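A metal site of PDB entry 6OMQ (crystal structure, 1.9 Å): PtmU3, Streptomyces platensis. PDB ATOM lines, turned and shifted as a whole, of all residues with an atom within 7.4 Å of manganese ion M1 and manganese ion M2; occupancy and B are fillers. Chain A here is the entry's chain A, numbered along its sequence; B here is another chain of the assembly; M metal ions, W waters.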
ATOM      1  N   ALA A   9      26.570   0.272 -37.430  1.00  0.00           N
ATOM      2  CA  ALA A   9      26.788  -1.151 -37.763  1.00  0.00           C
ATOM      3  C   ALA A   9      26.114  -2.108 -36.763  1.00  0.00           C
ATOM      4  O   ALA A   9      26.280  -3.340 -36.975  1.00  0.00           O
ATOM      5  CB  ALA A   9      28.265  -1.437 -37.867  1.00  0.00           C
ATOM      6  N   ASP A  10      25.264  -1.636 -35.840  1.00  0.00           N
ATOM      7  CA  ASP A  10      24.638  -2.545 -34.863  1.00  0.00           C
ATOM      8  C   ASP A  10      23.419  -1.949 -34.170  1.00  0.00           C
ATOM      9  O   ASP A  10      23.517  -0.834 -33.582  1.00  0.00           O
ATOM     10  CB  ASP A  10      25.726  -2.900 -33.845  1.00  0.00           C
ATOM     11  CG  ASP A  10      25.264  -3.864 -32.763  1.00  0.00           C
ATOM     12  OD1 ASP A  10      24.249  -4.538 -32.973  1.00  0.00           O
ATOM     13  OD2 ASP A  10      25.918  -3.907 -31.725  1.00  0.00           O
ATOM     14  N   SER A  11      22.354  -2.728 -34.225  1.00  0.00           N
ATOM     15  CA  SER A  11      21.087  -2.519 -33.508  1.00  0.00           C
ATOM     16  C   SER A  11      20.308  -3.818 -33.562  1.00  0.00           C
ATOM     17  O   SER A  11      20.689  -4.706 -34.287  1.00  0.00           O
ATOM     18  CB  SER A  11      20.280  -1.340 -34.103  1.00  0.00           C
ATOM     19  OG  SER A  11      19.742  -1.753 -35.346  1.00  0.00           O
ATOM     20  N   HIS A  12      19.236  -3.887 -32.782  1.00  0.00           N
ATOM     21  CA  HIS A  12      18.397  -5.072 -32.614  1.00  0.00           C
ATOM     22  C   HIS A  12      16.922  -4.679 -32.848  1.00  0.00           C
ATOM     23  O   HIS A  12      16.563  -3.530 -32.501  1.00  0.00           O
ATOM     24  CB  HIS A  12      18.630  -5.714 -31.247  1.00  0.00           C
ATOM     25  CG  HIS A  12      20.064  -6.092 -31.083  1.00  0.00           C
ATOM     26  ND1 HIS A  12      20.535  -7.336 -31.396  1.00  0.00           N
ATOM     27  CD2 HIS A  12      21.139  -5.350 -30.793  1.00  0.00           C
ATOM     28  CE1 HIS A  12      21.850  -7.350 -31.250  1.00  0.00           C
ATOM     29  NE2 HIS A  12      22.236  -6.143 -30.888  1.00  0.00           N
ATOM     30  N   PHE A  88      20.001  -6.521 -36.317  1.00  0.00           N
ATOM     31  CA  PHE A  88      20.212  -7.926 -35.895  1.00  0.00           C
ATOM     32  C   PHE A  88      18.964  -8.406 -35.170  1.00  0.00           C
ATOM     33  O   PHE A  88      18.207  -7.623 -34.643  1.00  0.00           O
ATOM     34  CB  PHE A  88      21.393  -8.019 -34.921  1.00  0.00           C
ATOM     35  CG  PHE A  88      22.719  -7.829 -35.591  1.00  0.00           C
ATOM     36  CD1 PHE A  88      23.246  -8.833 -36.355  1.00  0.00           C
ATOM     37  CD2 PHE A  88      23.404  -6.633 -35.505  1.00  0.00           C
ATOM     38  CE1 PHE A  88      24.454  -8.633 -37.021  1.00  0.00           C
ATOM     39  CE2 PHE A  88      24.626  -6.458 -36.135  1.00  0.00           C
ATOM     40  CZ  PHE A  88      25.136  -7.444 -36.914  1.00  0.00           C
ATOM     41  N   PRO A  89      18.791  -9.742 -35.039  1.00  0.00           N
ATOM     42  CA  PRO A  89      17.663 -10.297 -34.291  1.00  0.00           C
ATOM     43  C   PRO A  89      17.771 -10.025 -32.783  1.00  0.00           C
ATOM     44  O   PRO A  89      18.785  -9.538 -32.302  1.00  0.00           O
ATOM     45  CB  PRO A  89      17.737 -11.799 -34.575  1.00  0.00           C
ATOM     46  CG  PRO A  89      18.713 -11.979 -35.726  1.00  0.00           C
ATOM     47  CD  PRO A  89      19.591 -10.758 -35.737  1.00  0.00           C
ATOM     48  N   LEU A  93      17.983 -14.706 -32.087  1.00  0.00           N
ATOM     49  CA  LEU A  93      19.378 -15.075 -31.713  1.00  0.00           C
ATOM     50  C   LEU A  93      19.360 -16.455 -31.045  1.00  0.00           C
ATOM     51  O   LEU A  93      20.353 -17.198 -31.169  1.00  0.00           O
ATOM     52  CB  LEU A  93      19.967 -14.030 -30.752  1.00  0.00           C
ATOM     53  CG  LEU A  93      20.177 -12.617 -31.308  1.00  0.00           C
ATOM     54  CD1 LEU A  93      20.734 -11.688 -30.249  1.00  0.00           C
ATOM     55  CD2 LEU A  93      21.035 -12.608 -32.550  1.00  0.00           C
ATOM     56  N   HIS A 189      27.922 -11.725 -34.194  1.00  0.00           N
ATOM     57  CA  HIS A 189      27.499 -10.878 -33.062  1.00  0.00           C
ATOM     58  C   HIS A 189      27.839 -11.571 -31.751  1.00  0.00           C
ATOM     59  O   HIS A 189      27.472 -12.744 -31.553  1.00  0.00           O
ATOM     60  CB  HIS A 189      26.028 -10.479 -33.162  1.00  0.00           C
ATOM     61  CG  HIS A 189      25.658  -9.383 -32.219  1.00  0.00           C
ATOM     62  ND1 HIS A 189      25.677  -9.520 -30.855  1.00  0.00           N
ATOM     63  CD2 HIS A 189      25.237  -8.129 -32.464  1.00  0.00           C
ATOM     64  CE1 HIS A 189      25.349  -8.376 -30.298  1.00  0.00           C
ATOM     65  NE2 HIS A 189      25.055  -7.504 -31.279  1.00  0.00           N
ATOM     66  N   ILE A 190      28.414 -10.819 -30.812  1.00  0.00           N
ATOM     67  CA  ILE A 190      28.822 -11.439 -29.527  1.00  0.00           C
ATOM     68  C   ILE A 190      27.605 -11.709 -28.643  1.00  0.00           C
ATOM     69  O   ILE A 190      26.508 -11.205 -28.898  1.00  0.00           O
ATOM     70  CB  ILE A 190      29.908 -10.633 -28.777  1.00  0.00           C
ATOM     71  CG1 ILE A 190      29.540  -9.179 -28.513  1.00  0.00           C
ATOM     72  CG2 ILE A 190      31.241 -10.741 -29.497  1.00  0.00           C
ATOM     73  CD1 ILE A 190      28.633  -8.992 -27.361  1.00  0.00           C
ATOM     74  N   TYR A 209      30.485  -9.075 -18.777  1.00  0.00           N
ATOM     75  CA  TYR A 209      30.538  -8.231 -19.986  1.00  0.00           C
ATOM     76  C   TYR A 209      31.869  -8.446 -20.712  1.00  0.00           C
ATOM     77  O   TYR A 209      31.923  -8.453 -21.991  1.00  0.00           O
ATOM     78  CB  TYR A 209      30.296  -6.773 -19.604  1.00  0.00           C
ATOM     79  CG  TYR A 209      29.898  -5.931 -20.786  1.00  0.00           C
ATOM     80  CD1 TYR A 209      28.725  -6.185 -21.500  1.00  0.00           C
ATOM     81  CD2 TYR A 209      30.699  -4.897 -21.223  1.00  0.00           C
ATOM     82  CE1 TYR A 209      28.374  -5.425 -22.617  1.00  0.00           C
ATOM     83  CE2 TYR A 209      30.346  -4.122 -22.307  1.00  0.00           C
ATOM     84  CZ  TYR A 209      29.170  -4.368 -23.010  1.00  0.00           C
ATOM     85  OH  TYR A 209      28.877  -3.576 -24.110  1.00  0.00           O
ATOM     86  N   ALA A 240      30.474  -7.858 -34.442  1.00  0.00           N
ATOM     87  CA  ALA A 240      29.533  -6.835 -33.941  1.00  0.00           C
ATOM     88  C   ALA A 240      29.531  -6.830 -32.417  1.00  0.00           C
ATOM     89  O   ALA A 240      29.365  -7.913 -31.814  1.00  0.00           O
ATOM     90  CB  ALA A 240      28.174  -7.095 -34.518  1.00  0.00           C
ATOM     91  N   GLU A 241      29.721  -5.633 -31.831  1.00  0.00           N
ATOM     92  CA  GLU A 241      29.483  -5.284 -30.395  1.00  0.00           C
ATOM     93  C   GLU A 241      30.575  -5.901 -29.487  1.00  0.00           C
ATOM     94  O   GLU A 241      30.279  -6.190 -28.311  1.00  0.00           O
ATOM     95  CB  GLU A 241      28.090  -5.743 -29.940  1.00  0.00           C
ATOM     96  CG  GLU A 241      27.554  -4.952 -28.768  1.00  0.00           C
ATOM     97  CD  GLU A 241      26.276  -5.390 -28.095  1.00  0.00           C
ATOM     98  OE1 GLU A 241      25.237  -5.650 -28.786  1.00  0.00           O
ATOM     99  OE2 GLU A 241      26.249  -5.345 -26.853  1.00  0.00           O
ATOM    100  N   SER A 284      32.753  -3.458 -34.610  1.00  0.00           N
ATOM    101  CA  SER A 284      31.899  -2.331 -34.213  1.00  0.00           C
ATOM    102  C   SER A 284      32.103  -2.029 -32.732  1.00  0.00           C
ATOM    103  O   SER A 284      32.546  -2.932 -31.932  1.00  0.00           O
ATOM    104  CB  SER A 284      30.461  -2.595 -34.527  1.00  0.00           C
ATOM    105  OG  SER A 284      29.834  -3.410 -33.544  1.00  0.00           O
ATOM    106  N   GLN A 286      30.445   1.118 -29.553  1.00  0.00           N
ATOM    107  CA  GLN A 286      29.431   2.140 -29.188  1.00  0.00           C
ATOM    108  C   GLN A 286      30.141   3.319 -28.516  1.00  0.00           C
ATOM    109  O   GLN A 286      29.948   4.453 -28.969  1.00  0.00           O
ATOM    110  CB  GLN A 286      28.291   1.588 -28.333  1.00  0.00           C
ATOM    111  CG  GLN A 286      27.607   0.369 -28.921  1.00  0.00           C
ATOM    112  CD  GLN A 286      28.190  -0.931 -28.362  1.00  0.00           C
ATOM    113  OE1 GLN A 286      28.104  -1.184 -27.140  1.00  0.00           O
ATOM    114  NE2 GLN A 286      28.835  -1.707 -29.210  1.00  0.00           N
ATOM    115  N   SER A 307      25.279   1.927 -32.763  1.00  0.00           N
ATOM    116  CA  SER A 307      24.475   2.505 -31.660  1.00  0.00           C
ATOM    117  C   SER A 307      24.151   1.434 -30.624  1.00  0.00           C
ATOM    118  O   SER A 307      23.866   1.828 -29.496  1.00  0.00           O
ATOM    119  CB  SER A 307      23.167   3.130 -32.171  1.00  0.00           C
ATOM    120  OG  SER A 307      22.227   2.159 -32.503  1.00  0.00           O
ATOM    121  N   ASP A 308      23.963   0.208 -31.087  1.00  0.00           N
ATOM    122  CA  ASP A 308      23.424  -0.964 -30.338  1.00  0.00           C
ATOM    123  C   ASP A 308      22.057  -0.605 -29.750  1.00  0.00           C
ATOM    124  O   ASP A 308      21.674  -1.145 -28.719  1.00  0.00           O
ATOM    125  CB  ASP A 308      24.409  -1.558 -29.303  1.00  0.00           C
ATOM    126  CG  ASP A 308      24.005  -2.968 -28.868  1.00  0.00           C
ATOM    127  OD1 ASP A 308      23.744  -3.856 -29.771  1.00  0.00           O
ATOM    128  OD2 ASP A 308      24.076  -3.217 -27.651  1.00  0.00           O
ATOM    129  N   TYR A 309      21.272   0.195 -30.466  1.00  0.00           N
ATOM    130  CA  TYR A 309      19.857   0.425 -30.122  1.00  0.00           C
ATOM    131  C   TYR A 309      19.125  -0.905 -30.077  1.00  0.00           C
ATOM    132  O   TYR A 309      19.277  -1.768 -30.953  1.00  0.00           O
ATOM    133  CB  TYR A 309      19.216   1.354 -31.144  1.00  0.00           C
ATOM    134  CG  TYR A 309      17.785   1.725 -30.871  1.00  0.00           C
ATOM    135  CD1 TYR A 309      16.731   0.927 -31.276  1.00  0.00           C
ATOM    136  CD2 TYR A 309      17.492   2.934 -30.248  1.00  0.00           C
ATOM    137  CE1 TYR A 309      15.410   1.341 -31.095  1.00  0.00           C
ATOM    138  CE2 TYR A 309      16.186   3.358 -30.071  1.00  0.00           C
ATOM    139  CZ  TYR A 309      15.143   2.559 -30.488  1.00  0.00           C
ATOM    140  OH  TYR A 309      13.857   3.001 -30.285  1.00  0.00           O
ATOM    141  N   PRO A 310      18.233  -1.168 -29.120  1.00  0.00           N
ATOM    142  CA  PRO A 310      17.935  -0.332 -27.963  1.00  0.00           C
ATOM    143  C   PRO A 310      18.521  -0.858 -26.651  1.00  0.00           C
ATOM    144  O   PRO A 310      17.895  -0.713 -25.636  1.00  0.00           O
ATOM    145  CB  PRO A 310      16.399  -0.510 -27.941  1.00  0.00           C
ATOM    146  CG  PRO A 310      16.210  -1.974 -28.271  1.00  0.00           C
ATOM    147  CD  PRO A 310      17.367  -2.341 -29.173  1.00  0.00           C
ATOM    148  N   HIS A 311      19.706  -1.460 -26.709  1.00  0.00           N
ATOM    149  CA  HIS A 311      20.330  -2.153 -25.554  1.00  0.00           C
ATOM    150  C   HIS A 311      20.903  -1.105 -24.598  1.00  0.00           C
ATOM    151  O   HIS A 311      21.314  -0.014 -25.043  1.00  0.00           O
ATOM    152  CB  HIS A 311      21.387  -3.178 -25.995  1.00  0.00           C
ATOM    153  CG  HIS A 311      20.846  -4.383 -26.666  1.00  0.00           C
ATOM    154  ND1 HIS A 311      21.670  -5.267 -27.302  1.00  0.00           N
ATOM    155  CD2 HIS A 311      19.574  -4.832 -26.882  1.00  0.00           C
ATOM    156  CE1 HIS A 311      20.973  -6.267 -27.780  1.00  0.00           C
ATOM    157  NE2 HIS A 311      19.648  -5.982 -27.574  1.00  0.00           N
ATOM    158  N   LEU A 312      20.921  -1.444 -23.297  1.00  0.00           N
ATOM    159  CA  LEU A 312      21.536  -0.584 -22.250  1.00  0.00           C
ATOM    160  C   LEU A 312      22.935  -0.149 -22.697  1.00  0.00           C
ATOM    161  O   LEU A 312      23.271   1.003 -22.491  1.00  0.00           O
ATOM    162  CB  LEU A 312      21.617  -1.362 -20.919  1.00  0.00           C
ATOM    163  CG  LEU A 312      20.275  -1.606 -20.216  1.00  0.00           C
ATOM    164  CD1 LEU A 312      20.459  -2.542 -19.008  1.00  0.00           C
ATOM    165  CD2 LEU A 312      19.659  -0.289 -19.784  1.00  0.00           C
ATOM    166  N   GLU A 313      23.716  -1.045 -23.290  1.00  0.00           N
ATOM    167  CA  GLU A 313      25.142  -0.766 -23.619  1.00  0.00           C
ATOM    168  C   GLU A 313      25.260   0.086 -24.889  1.00  0.00           C
ATOM    169  O   GLU A 313      26.366   0.495 -25.242  1.00  0.00           O
ATOM    170  CB  GLU A 313      25.969  -2.038 -23.683  1.00  0.00           C
ATOM    171  CG  GLU A 313      25.471  -3.087 -24.640  1.00  0.00           C
ATOM    172  CD  GLU A 313      24.369  -4.045 -24.204  1.00  0.00           C
ATOM    173  OE1 GLU A 313      23.761  -3.861 -23.160  1.00  0.00           O
ATOM    174  OE2 GLU A 313      24.024  -4.923 -25.019  1.00  0.00           O
ATOM    175  N   GLY A 314      24.166   0.401 -25.552  1.00  0.00           N
ATOM    176  CA  GLY A 314      24.189   1.359 -26.663  1.00  0.00           C
ATOM    177  C   GLY A 314      24.163   2.802 -26.209  1.00  0.00           C
ATOM    178  O   GLY A 314      24.173   3.092 -24.985  1.00  0.00           O
ATOM    179  N   HIS B 261      25.540  -0.554 -17.358  1.00  0.00           N
ATOM    180  CA  HIS B 261      24.938  -1.684 -16.598  1.00  0.00           C
ATOM    181  C   HIS B 261      25.030  -1.410 -15.096  1.00  0.00           C
ATOM    182  O   HIS B 261      24.932  -2.405 -14.331  1.00  0.00           O
ATOM    183  CB  HIS B 261      25.585  -3.022 -16.916  1.00  0.00           C
ATOM    184  CG  HIS B 261      25.372  -3.495 -18.310  1.00  0.00           C
ATOM    185  ND1 HIS B 261      25.961  -4.634 -18.755  1.00  0.00           N
ATOM    186  CD2 HIS B 261      24.641  -2.982 -19.350  1.00  0.00           C
ATOM    187  CE1 HIS B 261      25.587  -4.858 -20.005  1.00  0.00           C
ATOM    188  NE2 HIS B 261      24.769  -3.826 -20.416  1.00  0.00           N
HETATM  189 MN    MN M   1      24.336  -5.365 -30.822  1.00  0.00          MN
HETATM  190 MN    MN M   2      23.894  -5.307 -27.068  1.00  0.00          MN
HETATM  191  O   HOH W   1      23.722  -7.646 -26.931  1.00  0.00           O
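OD1 of Asp 308 is bound to manganese ion M1. A ring nitrogen (NE2) of His 12 is bound to manganese ion M1 (2.2 Å). Manganese ion M1 is bound by OE1 of Glu 241, at 2.2 Å. Manganese ion M1 is bound by a ring nitrogen (NE2) of His 189 (2.3 Å). Manganese ion M1 is bound by the side-chain carboxylate (OD1) of Asp 10. OD2 of Asp 10 is bound to manganese ion M1 (2.3 Å). Manganese ion M1 has six donor atoms within binding distance.
Within 4 Å of manganese ion M1: Asp 10, His 12, His 189, Glu 241 and Asp 308. Along chain A the residues within 4 Å of manganese ion M1 span positions 10 to 308. The nearest printed residue that does not touch manganese ion M1 is His 311 (4.4 Å).
Manganese ion M2 is bound by OE2 of Glu 313, at 2.1 Å. The side-chain carboxylate (OD2) of Asp 308 is bound to manganese ion M2 (2.2 Å). Manganese ion M2 is bound by OE1 of Glu 241 (2.2 Å). Manganese ion M2 is bound by ND1 of His 311 (2.2 Å). Water W1 is bound to manganese ion M2, at 2.3 Å. Manganese ion M2 is bound by OE2 of Glu 241, at 2.4 Å.
The side-chain amide oxygen (OE1) of Gln 286 lies close to the backbone carbonyl oxygen (O) of Glu 313. OE1 of Glu 313 lies within hydrogen-bond range of NE2 of His 261 of chain B, at 2.9 Å. The side-chain hydroxyl (OG) of Ser 284 lies within hydrogen-bond range of the backbone NH (N) of Glu 241 (2.8 Å). O of Tyr 309 is in hydrogen-bond range of N of His 12 (2.8 Å). The backbone carbonyl oxygen (O) of Pro 89 lies within hydrogen-bond range of a ring nitrogen (ND1) of His 12 (3.0 Å). The backbone carbonyl oxygen (O) of Asp 10 lies within hydrogen-bond range of the backbone NH (N) of Ser 307, 3.4 Å away.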
